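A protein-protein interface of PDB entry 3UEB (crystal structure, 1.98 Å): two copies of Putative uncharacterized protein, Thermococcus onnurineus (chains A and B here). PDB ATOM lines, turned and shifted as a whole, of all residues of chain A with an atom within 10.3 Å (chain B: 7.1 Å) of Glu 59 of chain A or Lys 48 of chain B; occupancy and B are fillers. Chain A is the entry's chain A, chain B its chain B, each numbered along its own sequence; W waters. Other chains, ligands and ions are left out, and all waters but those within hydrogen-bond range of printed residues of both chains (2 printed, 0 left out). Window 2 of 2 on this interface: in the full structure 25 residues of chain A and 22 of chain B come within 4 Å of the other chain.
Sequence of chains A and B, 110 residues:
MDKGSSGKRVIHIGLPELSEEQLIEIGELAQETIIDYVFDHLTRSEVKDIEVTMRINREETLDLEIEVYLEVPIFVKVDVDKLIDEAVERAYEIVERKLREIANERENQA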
ATOM      1  N   ILE A  13      13.580  12.749 -32.229  1.00  0.00           N
ATOM      2  CA  ILE A  13      12.929  11.479 -32.513  1.00  0.00           C
ATOM      3  C   ILE A  13      11.638  11.245 -31.724  1.00  0.00           C
ATOM      4  O   ILE A  13      11.597  11.416 -30.499  1.00  0.00           O
ATOM      5  CB  ILE A  13      13.895  10.307 -32.232  1.00  0.00           C
ATOM      6  CG1 ILE A  13      15.173  10.471 -33.064  1.00  0.00           C
ATOM      7  CG2 ILE A  13      13.225   8.984 -32.571  1.00  0.00           C
ATOM      8  CD1 ILE A  13      16.218   9.376 -32.831  1.00  0.00           C
ATOM      9  N   GLU A  20       7.744   4.924 -21.611  1.00  0.00           N
ATOM     10  CA  GLU A  20       8.852   5.804 -21.239  1.00  0.00           C
ATOM     11  C   GLU A  20      10.128   5.028 -20.901  1.00  0.00           C
ATOM     12  O   GLU A  20      11.237   5.512 -21.135  1.00  0.00           O
ATOM     13  CB  GLU A  20       8.434   6.738 -20.090  1.00  0.00           C
ATOM     14  CG  GLU A  20       7.479   7.847 -20.568  1.00  0.00           C
ATOM     15  CD  GLU A  20       6.949   8.730 -19.449  1.00  0.00           C
ATOM     16  OE1 GLU A  20       6.328   8.187 -18.511  1.00  0.00           O
ATOM     17  OE2 GLU A  20       7.143   9.968 -19.514  1.00  0.00           O
ATOM     18  N   LEU A  23      11.921   4.068 -23.892  1.00  0.00           N
ATOM     19  CA  LEU A  23      12.439   5.304 -24.456  1.00  0.00           C
ATOM     20  C   LEU A  23      13.879   5.497 -23.973  1.00  0.00           C
ATOM     21  O   LEU A  23      14.753   5.915 -24.738  1.00  0.00           O
ATOM     22  CB  LEU A  23      11.564   6.474 -24.006  1.00  0.00           C
ATOM     23  CG  LEU A  23      11.373   7.649 -24.961  1.00  0.00           C
ATOM     24  CD1 LEU A  23      10.841   7.147 -26.310  1.00  0.00           C
ATOM     25  CD2 LEU A  23      10.390   8.625 -24.340  1.00  0.00           C
ATOM     26  N   ILE A  24      14.114   5.198 -22.698  1.00  0.00           N
ATOM     27  CA  ILE A  24      15.446   5.311 -22.102  1.00  0.00           C
ATOM     28  C   ILE A  24      16.376   4.325 -22.807  1.00  0.00           C
ATOM     29  O   ILE A  24      17.490   4.673 -23.203  1.00  0.00           O
ATOM     30  CB  ILE A  24      15.415   4.982 -20.571  1.00  0.00           C
ATOM     31  CG1 ILE A  24      15.014   6.223 -19.771  1.00  0.00           C
ATOM     32  CG2 ILE A  24      16.773   4.475 -20.096  1.00  0.00           C
ATOM     33  CD1 ILE A  24      13.601   6.686 -20.017  1.00  0.00           C
ATOM     34  N   ARG A  55      18.388  13.238 -24.474  1.00  0.00           N
ATOM     35  CA  ARG A  55      17.400  13.960 -23.690  1.00  0.00           C
ATOM     36  C   ARG A  55      16.050  13.259 -23.817  1.00  0.00           C
ATOM     37  O   ARG A  55      15.520  13.123 -24.918  1.00  0.00           O
ATOM     38  CB  ARG A  55      17.276  15.404 -24.191  1.00  0.00           C
ATOM     39  CG  ARG A  55      16.183  16.204 -23.487  1.00  0.00           C
ATOM     40  CD  ARG A  55      15.917  17.546 -24.165  1.00  0.00           C
ATOM     41  NE  ARG A  55      14.880  18.311 -23.472  1.00  0.00           N
ATOM     42  CZ  ARG A  55      14.321  19.425 -23.944  1.00  0.00           C
ATOM     43  NH1 ARG A  55      13.387  20.053 -23.237  1.00  0.00           N
ATOM     44  NH2 ARG A  55      14.689  19.909 -25.126  1.00  0.00           N
ATOM     45  N   ILE A  56      15.503  12.803 -22.695  1.00  0.00           N
ATOM     46  CA  ILE A  56      14.207  12.132 -22.712  1.00  0.00           C
ATOM     47  C   ILE A  56      13.171  13.030 -22.045  1.00  0.00           C
ATOM     48  O   ILE A  56      13.303  13.400 -20.877  1.00  0.00           O
ATOM     49  CB  ILE A  56      14.255  10.755 -21.990  1.00  0.00           C
ATOM     50  CG1 ILE A  56      14.965   9.713 -22.868  1.00  0.00           C
ATOM     51  CG2 ILE A  56      12.841  10.264 -21.696  1.00  0.00           C
ATOM     52  CD1 ILE A  56      16.458   9.904 -22.999  1.00  0.00           C
ATOM     53  N   ASN A  57      12.142  13.387 -22.801  1.00  0.00           N
ATOM     54  CA  ASN A  57      11.092  14.254 -22.291  1.00  0.00           C
ATOM     55  C   ASN A  57       9.848  14.082 -23.160  1.00  0.00           C
ATOM     56  O   ASN A  57       9.636  14.830 -24.117  1.00  0.00           O
ATOM     57  CB  ASN A  57      11.561  15.711 -22.331  1.00  0.00           C
ATOM     58  CG  ASN A  57      10.595  16.656 -21.645  1.00  0.00           C
ATOM     59  OD1 ASN A  57       9.380  16.415 -21.618  1.00  0.00           O
ATOM     60  ND2 ASN A  57      11.125  17.747 -21.096  1.00  0.00           N
ATOM     61  N   ARG A  58       9.027  13.096 -22.819  1.00  0.00           N
ATOM     62  CA  ARG A  58       7.813  12.818 -23.574  1.00  0.00           C
ATOM     63  C   ARG A  58       6.758  13.927 -23.540  1.00  0.00           C
ATOM     64  O   ARG A  58       6.006  14.102 -24.493  1.00  0.00           O
ATOM     65  CB  ARG A  58       7.191  11.505 -23.090  1.00  0.00           C
ATOM     66  CG  ARG A  58       5.796  11.246 -23.654  1.00  0.00           C
ATOM     67  CD  ARG A  58       5.505   9.754 -23.764  1.00  0.00           C
ATOM     68  NE  ARG A  58       6.318   9.115 -24.797  1.00  0.00           N
ATOM     69  CZ  ARG A  58       6.356   7.803 -25.008  1.00  0.00           C
ATOM     70  NH1 ARG A  58       5.631   6.985 -24.252  1.00  0.00           N
ATOM     71  NH2 ARG A  58       7.104   7.304 -25.985  1.00  0.00           N
ATOM     72  N   GLU A  59       6.701  14.689 -22.456  1.00  0.00           N
ATOM     73  CA  GLU A  59       5.695  15.735 -22.362  1.00  0.00           C
ATOM     74  C   GLU A  59       5.980  17.068 -23.044  1.00  0.00           C
ATOM     75  O   GLU A  59       5.047  17.816 -23.329  1.00  0.00           O
ATOM     76  CB  GLU A  59       5.329  15.974 -20.901  1.00  0.00           C
ATOM     77  CG  GLU A  59       4.454  14.863 -20.337  1.00  0.00           C
ATOM     78  CD  GLU A  59       3.293  15.396 -19.529  1.00  0.00           C
ATOM     79  OE1 GLU A  59       3.539  15.919 -18.423  1.00  0.00           O
ATOM     80  OE2 GLU A  59       2.137  15.299 -20.006  1.00  0.00           O
ATOM     81  N   GLU A  60       7.245  17.369 -23.329  1.00  0.00           N
ATOM     82  CA  GLU A  60       7.566  18.644 -23.970  1.00  0.00           C
ATOM     83  C   GLU A  60       8.316  18.535 -25.299  1.00  0.00           C
ATOM     84  O   GLU A  60       8.588  19.549 -25.940  1.00  0.00           O
ATOM     85  CB  GLU A  60       8.365  19.526 -22.999  1.00  0.00           C
ATOM     86  CG  GLU A  60       7.625  19.872 -21.705  1.00  0.00           C
ATOM     87  CD  GLU A  60       8.531  20.520 -20.662  1.00  0.00           C
ATOM     88  OE1 GLU A  60       9.491  19.862 -20.203  1.00  0.00           O
ATOM     89  OE2 GLU A  60       8.288  21.690 -20.297  1.00  0.00           O
ATOM     90  N   THR A  61       8.654  17.319 -25.717  1.00  0.00           N
ATOM     91  CA  THR A  61       9.369  17.130 -26.985  1.00  0.00           C
ATOM     92  C   THR A  61       8.758  15.957 -27.753  1.00  0.00           C
ATOM     93  O   THR A  61       7.764  15.373 -27.318  1.00  0.00           O
ATOM     94  CB  THR A  61      10.890  16.820 -26.764  1.00  0.00           C
ATOM     95  OG1 THR A  61      11.056  15.473 -26.304  1.00  0.00           O
ATOM     96  CG2 THR A  61      11.489  17.757 -25.740  1.00  0.00           C
ATOM     97  N   LEU A  62       9.353  15.615 -28.890  1.00  0.00           N
ATOM     98  CA  LEU A  62       8.869  14.490 -29.672  1.00  0.00           C
ATOM     99  C   LEU A  62       9.018  13.219 -28.838  1.00  0.00           C
ATOM    100  O   LEU A  62       8.281  12.256 -29.029  1.00  0.00           O
ATOM    101  CB  LEU A  62       9.666  14.361 -30.974  1.00  0.00           C
ATOM    102  CG  LEU A  62       9.001  14.929 -32.234  1.00  0.00           C
ATOM    103  CD1 LEU A  62       8.712  16.411 -32.055  1.00  0.00           C
ATOM    104  CD2 LEU A  62       9.912  14.699 -33.432  1.00  0.00           C
ATOM    105  N   ASP A  63       9.980  13.240 -27.915  1.00  0.00           N
ATOM    106  CA  ASP A  63      10.271  12.127 -27.007  1.00  0.00           C
ATOM    107  C   ASP A  63      11.752  12.061 -26.702  1.00  0.00           C
ATOM    108  O   ASP A  63      12.171  12.186 -25.549  1.00  0.00           O
ATOM    109  CB  ASP A  63       9.857  10.775 -27.602  1.00  0.00           C
ATOM    110  CG  ASP A  63       8.430  10.395 -27.259  1.00  0.00           C
ATOM    111  OD1 ASP A  63       7.925   9.419 -27.856  1.00  0.00           O
ATOM    112  OD2 ASP A  63       7.824  11.065 -26.392  1.00  0.00           O
ATOM    113  N   LEU A  64      12.539  11.853 -27.751  1.00  0.00           N
ATOM    114  CA  LEU A  64      13.971  11.735 -27.608  1.00  0.00           C
ATOM    115  C   LEU A  64      14.712  12.739 -28.465  1.00  0.00           C
ATOM    116  O   LEU A  64      14.337  13.007 -29.609  1.00  0.00           O
ATOM    117  CB  LEU A  64      14.407  10.313 -27.978  1.00  0.00           C
ATOM    118  CG  LEU A  64      15.908   9.998 -28.011  1.00  0.00           C
ATOM    119  CD1 LEU A  64      16.527  10.144 -26.611  1.00  0.00           C
ATOM    120  CD2 LEU A  64      16.091   8.582 -28.523  1.00  0.00           C
ATOM    121  N   GLU A  65      15.761  13.308 -27.892  1.00  0.00           N
ATOM    122  CA  GLU A  65      16.586  14.257 -28.605  1.00  0.00           C
ATOM    123  C   GLU A  65      18.018  13.812 -28.398  1.00  0.00           C
ATOM    124  O   GLU A  65      18.419  13.458 -27.290  1.00  0.00           O
ATOM    125  CB  GLU A  65      16.367  15.682 -28.087  1.00  0.00           C
ATOM    126  CG  GLU A  65      14.936  16.182 -28.298  1.00  0.00           C
ATOM    127  CD  GLU A  65      14.808  17.699 -28.250  1.00  0.00           C
ATOM    128  OE1 GLU A  65      13.687  18.210 -28.476  1.00  0.00           O
ATOM    129  OE2 GLU A  65      15.824  18.383 -27.993  1.00  0.00           O
ATOM    130  N   LYS B   3       7.597  25.321 -13.605  1.00  0.00           N
ATOM    131  CA  LYS B   3       8.868  24.533 -13.612  1.00  0.00           C
ATOM    132  C   LYS B   3       9.110  23.862 -12.262  1.00  0.00           C
ATOM    133  O   LYS B   3       9.354  24.535 -11.262  1.00  0.00           O
ATOM    134  CB  LYS B   3      10.045  25.443 -13.958  1.00  0.00           C
ATOM    135  N   GLY B   4       9.045  22.533 -12.244  1.00  0.00           N
ATOM    136  CA  GLY B   4       9.263  21.795 -11.011  1.00  0.00           C
ATOM    137  C   GLY B   4      10.718  21.766 -10.588  1.00  0.00           C
ATOM    138  O   GLY B   4      11.571  22.392 -11.223  1.00  0.00           O
ATOM    139  N   LEU B  42      12.670   6.756  -8.763  1.00  0.00           N
ATOM    140  CA  LEU B  42      11.545   7.526  -9.274  1.00  0.00           C
ATOM    141  C   LEU B  42      10.751   6.688 -10.263  1.00  0.00           C
ATOM    142  O   LEU B  42      11.286   5.772 -10.890  1.00  0.00           O
ATOM    143  CB  LEU B  42      12.029   8.789  -9.995  1.00  0.00           C
ATOM    144  CG  LEU B  42      12.601   9.961  -9.195  1.00  0.00           C
ATOM    145  CD1 LEU B  42      12.960  11.096 -10.148  1.00  0.00           C
ATOM    146  CD2 LEU B  42      11.575  10.440  -8.179  1.00  0.00           C
ATOM    147  N   THR B  43       9.469   6.997 -10.397  1.00  0.00           N
ATOM    148  CA  THR B  43       8.631   6.291 -11.356  1.00  0.00           C
ATOM    149  C   THR B  43       8.761   7.097 -12.643  1.00  0.00           C
ATOM    150  O   THR B  43       9.083   8.286 -12.598  1.00  0.00           O
ATOM    151  CB  THR B  43       7.159   6.246 -10.891  1.00  0.00           C
ATOM    152  OG1 THR B  43       6.719   7.567 -10.547  1.00  0.00           O
ATOM    153  CG2 THR B  43       7.020   5.345  -9.676  1.00  0.00           C
ATOM    154  N   ARG B  44       8.542   6.460 -13.786  1.00  0.00           N
ATOM    155  CA  ARG B  44       8.661   7.162 -15.059  1.00  0.00           C
ATOM    156  C   ARG B  44       7.836   8.450 -15.151  1.00  0.00           C
ATOM    157  O   ARG B  44       8.196   9.369 -15.889  1.00  0.00           O
ATOM    158  CB  ARG B  44       8.300   6.229 -16.217  1.00  0.00           C
ATOM    159  CG  ARG B  44       9.491   5.435 -16.757  1.00  0.00           C
ATOM    160  CD  ARG B  44      10.040   4.457 -15.736  1.00  0.00           C
ATOM    161  NE  ARG B  44      11.147   3.678 -16.285  1.00  0.00           N
ATOM    162  CZ  ARG B  44      11.771   2.697 -15.639  1.00  0.00           C
ATOM    163  NH1 ARG B  44      11.400   2.362 -14.409  1.00  0.00           N
ATOM    164  NH2 ARG B  44      12.769   2.050 -16.222  1.00  0.00           N
ATOM    165  N   SER B  45       6.750   8.532 -14.392  1.00  0.00           N
ATOM    166  CA  SER B  45       5.902   9.722 -14.419  1.00  0.00           C
ATOM    167  C   SER B  45       6.486  10.898 -13.652  1.00  0.00           C
ATOM    168  O   SER B  45       6.209  12.047 -13.975  1.00  0.00           O
ATOM    169  CB  SER B  45       4.518   9.391 -13.867  1.00  0.00           C
ATOM    170  OG  SER B  45       3.880   8.431 -14.694  1.00  0.00           O
ATOM    171  N   GLU B  46       7.287  10.614 -12.633  1.00  0.00           N
ATOM    172  CA  GLU B  46       7.896  11.674 -11.847  1.00  0.00           C
ATOM    173  C   GLU B  46       9.051  12.345 -12.584  1.00  0.00           C
ATOM    174  O   GLU B  46       9.532  13.399 -12.166  1.00  0.00           O
ATOM    175  CB  GLU B  46       8.395  11.121 -10.512  1.00  0.00           C
ATOM    176  CG  GLU B  46       7.292  10.542  -9.639  1.00  0.00           C
ATOM    177  CD  GLU B  46       7.819   9.904  -8.372  1.00  0.00           C
ATOM    178  OE1 GLU B  46       8.649   8.974  -8.474  1.00  0.00           O
ATOM    179  OE2 GLU B  46       7.400  10.332  -7.274  1.00  0.00           O
ATOM    180  N   VAL B  47       9.493  11.743 -13.683  1.00  0.00           N
ATOM    181  CA  VAL B  47      10.602  12.295 -14.452  1.00  0.00           C
ATOM    182  C   VAL B  47      10.110  13.039 -15.680  1.00  0.00           C
ATOM    183  O   VAL B  47       9.819  12.433 -16.712  1.00  0.00           O
ATOM    184  CB  VAL B  47      11.582  11.192 -14.906  1.00  0.00           C
ATOM    185  CG1 VAL B  47      12.728  11.807 -15.711  1.00  0.00           C
ATOM    186  CG2 VAL B  47      12.132  10.467 -13.696  1.00  0.00           C
ATOM    187  N   LYS B  48      10.026  14.359 -15.563  1.00  0.00           N
ATOM    188  CA  LYS B  48       9.579  15.185 -16.666  1.00  0.00           C
ATOM    189  C   LYS B  48      10.688  15.319 -17.699  1.00  0.00           C
ATOM    190  O   LYS B  48      10.458  15.216 -18.901  1.00  0.00           O
ATOM    191  CB  LYS B  48       9.187  16.577 -16.167  1.00  0.00           C
ATOM    192  CG  LYS B  48       8.513  17.424 -17.228  1.00  0.00           C
ATOM    193  CD  LYS B  48       8.085  18.760 -16.671  1.00  0.00           C
ATOM    194  CE  LYS B  48       7.153  19.470 -17.629  1.00  0.00           C
ATOM    195  NZ  LYS B  48       5.931  18.646 -17.880  1.00  0.00           N
ATOM    196  N   ASP B  49      11.899  15.545 -17.222  1.00  0.00           N
ATOM    197  CA  ASP B  49      13.019  15.710 -18.127  1.00  0.00           C
ATOM    198  C   ASP B  49      14.316  15.171 -17.528  1.00  0.00           C
ATOM    199  O   ASP B  49      14.659  15.451 -16.374  1.00  0.00           O
ATOM    200  CB  ASP B  49      13.160  17.198 -18.480  1.00  0.00           C
ATOM    201  CG  ASP B  49      14.213  17.460 -19.549  1.00  0.00           C
ATOM    202  OD1 ASP B  49      14.118  16.893 -20.653  1.00  0.00           O
ATOM    203  OD2 ASP B  49      15.135  18.248 -19.283  1.00  0.00           O
ATOM    204  N   ILE B  50      15.012  14.357 -18.310  1.00  0.00           N
ATOM    205  CA  ILE B  50      16.292  13.822 -17.898  1.00  0.00           C
ATOM    206  C   ILE B  50      17.211  13.978 -19.104  1.00  0.00           C
ATOM    207  O   ILE B  50      16.877  13.551 -20.212  1.00  0.00           O
ATOM    208  CB  ILE B  50      16.192  12.341 -17.455  1.00  0.00           C
ATOM    209  CG1 ILE B  50      17.553  11.874 -16.931  1.00  0.00           C
ATOM    210  CG2 ILE B  50      15.732  11.461 -18.605  1.00  0.00           C
ATOM    211  CD1 ILE B  50      17.512  10.560 -16.176  1.00  0.00           C
ATOM    212  N   LEU B  70      18.191  16.798 -14.349  1.00  0.00           N
ATOM    213  CA  LEU B  70      16.941  16.121 -14.053  1.00  0.00           C
ATOM    214  C   LEU B  70      15.917  17.142 -13.588  1.00  0.00           C
ATOM    215  O   LEU B  70      16.250  18.081 -12.872  1.00  0.00           O
ATOM    216  CB  LEU B  70      17.155  15.074 -12.958  1.00  0.00           C
ATOM    217  CG  LEU B  70      15.918  14.299 -12.507  1.00  0.00           C
ATOM    218  CD1 LEU B  70      15.388  13.440 -13.661  1.00  0.00           C
ATOM    219  CD2 LEU B  70      16.295  13.418 -11.329  1.00  0.00           C
ATOM    220  N   GLU B  71      14.674  16.939 -14.003  1.00  0.00           N
ATOM    221  CA  GLU B  71      13.576  17.820 -13.643  1.00  0.00           C
ATOM    222  C   GLU B  71      12.331  16.975 -13.418  1.00  0.00           C
ATOM    223  O   GLU B  71      12.039  16.072 -14.200  1.00  0.00           O
ATOM    224  CB  GLU B  71      13.327  18.808 -14.778  1.00  0.00           C
ATOM    225  CG  GLU B  71      12.286  19.866 -14.497  1.00  0.00           C
ATOM    226  CD  GLU B  71      11.976  20.690 -15.742  1.00  0.00           C
ATOM    227  OE1 GLU B  71      12.928  21.048 -16.470  1.00  0.00           O
ATOM    228  OE2 GLU B  71      10.786  20.982 -15.993  1.00  0.00           O
ATOM    229  N   VAL B  72      11.600  17.275 -12.348  1.00  0.00           N
ATOM    230  CA  VAL B  72      10.373  16.565 -12.018  1.00  0.00           C
ATOM    231  C   VAL B  72       9.199  17.540 -12.120  1.00  0.00           C
ATOM    232  O   VAL B  72       9.395  18.755 -12.116  1.00  0.00           O
ATOM    233  CB  VAL B  72      10.409  16.018 -10.569  1.00  0.00           C
ATOM    234  CG1 VAL B  72      11.606  15.123 -10.382  1.00  0.00           C
ATOM    235  CG2 VAL B  72      10.444  17.159  -9.578  1.00  0.00           C
ATOM    236  N   PRO B  73       7.961  17.019 -12.203  1.00  0.00           N
ATOM    237  CA  PRO B  73       6.796  17.914 -12.296  1.00  0.00           C
ATOM    238  C   PRO B  73       6.718  18.815 -11.061  1.00  0.00           C
ATOM    239  O   PRO B  73       7.179  18.443  -9.983  1.00  0.00           O
ATOM    240  CB  PRO B  73       5.617  16.942 -12.379  1.00  0.00           C
ATOM    241  CG  PRO B  73       6.227  15.734 -13.078  1.00  0.00           C
ATOM    242  CD  PRO B  73       7.563  15.608 -12.376  1.00  0.00           C
ATOM    243  N   ILE B  74       6.134  19.994 -11.216  1.00  0.00           N
ATOM    244  CA  ILE B  74       6.021  20.926 -10.105  1.00  0.00           C
ATOM    245  C   ILE B  74       5.262  20.357  -8.902  1.00  0.00           C
ATOM    246  O   ILE B  74       5.434  20.837  -7.780  1.00  0.00           O
ATOM    247  CB  ILE B  74       5.341  22.252 -10.547  1.00  0.00           C
ATOM    248  CG1 ILE B  74       5.337  23.252  -9.386  1.00  0.00           C
ATOM    249  CG2 ILE B  74       3.902  21.984 -10.998  1.00  0.00           C
ATOM    250  CD1 ILE B  74       6.698  23.465  -8.728  1.00  0.00           C
ATOM    251  N   PHE B  75       4.439  19.334  -9.121  1.00  0.00           N
ATOM    252  CA  PHE B  75       3.674  18.744  -8.019  1.00  0.00           C
ATOM    253  C   PHE B  75       4.362  17.552  -7.342  1.00  0.00           C
ATOM    254  O   PHE B  75       3.845  17.014  -6.363  1.00  0.00           O
ATOM    255  CB  PHE B  75       2.275  18.334  -8.508  1.00  0.00           C
ATOM    256  CG  PHE B  75       2.292  17.408  -9.694  1.00  0.00           C
ATOM    257  CD1 PHE B  75       2.508  16.045  -9.528  1.00  0.00           C
ATOM    258  CD2 PHE B  75       2.101  17.905 -10.983  1.00  0.00           C
ATOM    259  CE1 PHE B  75       2.532  15.186 -10.625  1.00  0.00           C
ATOM    260  CE2 PHE B  75       2.124  17.058 -12.086  1.00  0.00           C
ATOM    261  CZ  PHE B  75       2.340  15.695 -11.906  1.00  0.00           C
HETATM  262  O   HOH W   1       8.188  14.132 -19.860  1.00  0.00           O
HETATM  263  O   HOH W   2       4.477  16.114 -15.994  1.00  0.00           O
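Arg 55 of chain A touches Ile 50 of chain B (CA to O, 3.5 Å).
Ile 56 of chain A touches Lys 48 of chain B.
OD1 of Asp 49 of chain B touches O of Ile 56 of chain A, at 3.6 Å.
Lys 48 of chain B touches Glu 60 of chain A.
No position is printed for both chains.
Of the 10 pairs that touch across the chains among the printed residues, none has its exchanged pair printed and touching as well.
Water W2 bridges the side-chain carboxylate (OE1) of Glu 59 of chain A (2.6 Å) and the side-chain amino group (NZ) of Lys 48 of chain B (3.5 Å).
Water W1 lies within hydrogen-bond range of O of Lys 48 of chain B (2.7 Å), N of Glu 59 of chain A (3.0 Å), OD1 of Asn 57 of chain A (3.1 Å) and N of Arg 58 of chain A (3.2 Å).
The guanidinium group of Arg 55 of chain A lies within salt-bridge range of the side-chain carboxylate of Asp 49 of chain B (3.2 Å).
N of Ile 56 of chain A is in hydrogen-bond range of O of Ile 50 of chain B, 2.9 Å away.
The backbone carbonyl oxygen (O) of Lys 48 of chain B lies close to the side-chain amide oxygen (OD1) of Asn 57 of chain A, at 3.2 Å.
The side-chain carboxylate (OD1) of Asp 49 of chain B lies within hydrogen-bond range of the side-chain amide nitrogen (ND2) of Asn 57 of chain A (3.1 Å).
NZ of Lys 48 of chain B lies within salt-bridge range of OE1 of Glu 59 of chain A (3.7 Å).
OE1 of Glu 20 of chain A sits close to O of Arg 44 of chain B, 3.4 Å away.
Printed residues of chain B within 4 Å of Glu 59 of chain A: Lys 48.
Lys 48 of chain B touches just these residues of chain A: Ile 56 (3.9 Å), Asn 57 (3.1 Å), Glu 59 (3.7 Å) and Glu 60 (3.5 Å).
No residue of chain A comes within 4 Å of Val 47 of chain B.
Of chain A, only Arg 55 (3.2 Å), Ile 56 (3.6 Å) and Asn 57 (3.1 Å) come within 4 Å of Asp 49 of chain B.
Printed residues of chain B within 4 Å of Glu 60 of chain A: Lys 48 (3.5 Å).
Printed residues of chain A within 4 Å of Ile 50 of chain B: Arg 55 and Ile 56.
Leu 64 of chain A touches none of the printed residues of chain B.
Thr 61 of chain A touches none of the printed residues of chain B.
The guanidinium group (NH2) of Arg 55 of chain A is in salt-bridge range of the side-chain carboxylate (OE2) of Glu 65 of chain A.
The side-chain amide oxygen (OD1) of Asn 57 of chain A lies close to the backbone NH (N) of Glu 59 of chain A (3.3 Å).
The side-chain amide nitrogen (ND2) of Asn 57 of chain A sits at hydrogen-bond distance from the side-chain carboxylate (OE1) of Glu 60 of chain A, 2.8 Å away.
OG1 of Thr 61 of chain A lies within hydrogen-bond range of O of Asn 57 of chain A, at 2.7 Å.
N of Asn 57 of chain A is in hydrogen-bond range of O of Asp 63 of chain A, 3.0 Å away.
O of Glu 71 of chain B sits at hydrogen-bond distance from N of Lys 48 of chain B, 3.0 Å away.
Of the 15 printed residues of chain A, 6 touch a printed residue of chain B.
Hydrophobic or aromatic side chains of chain A within 4 Å of the printed part of chain B: Ile 56.
Along chain A the printed residues that touch a printed residue of chain B span positions 20 to 60.
Hydrophobic or aromatic side chains of chain B within 4 Å of the printed part of chain A: Ile 50.
Among the printed residues, 10 pairs touch across the chains.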
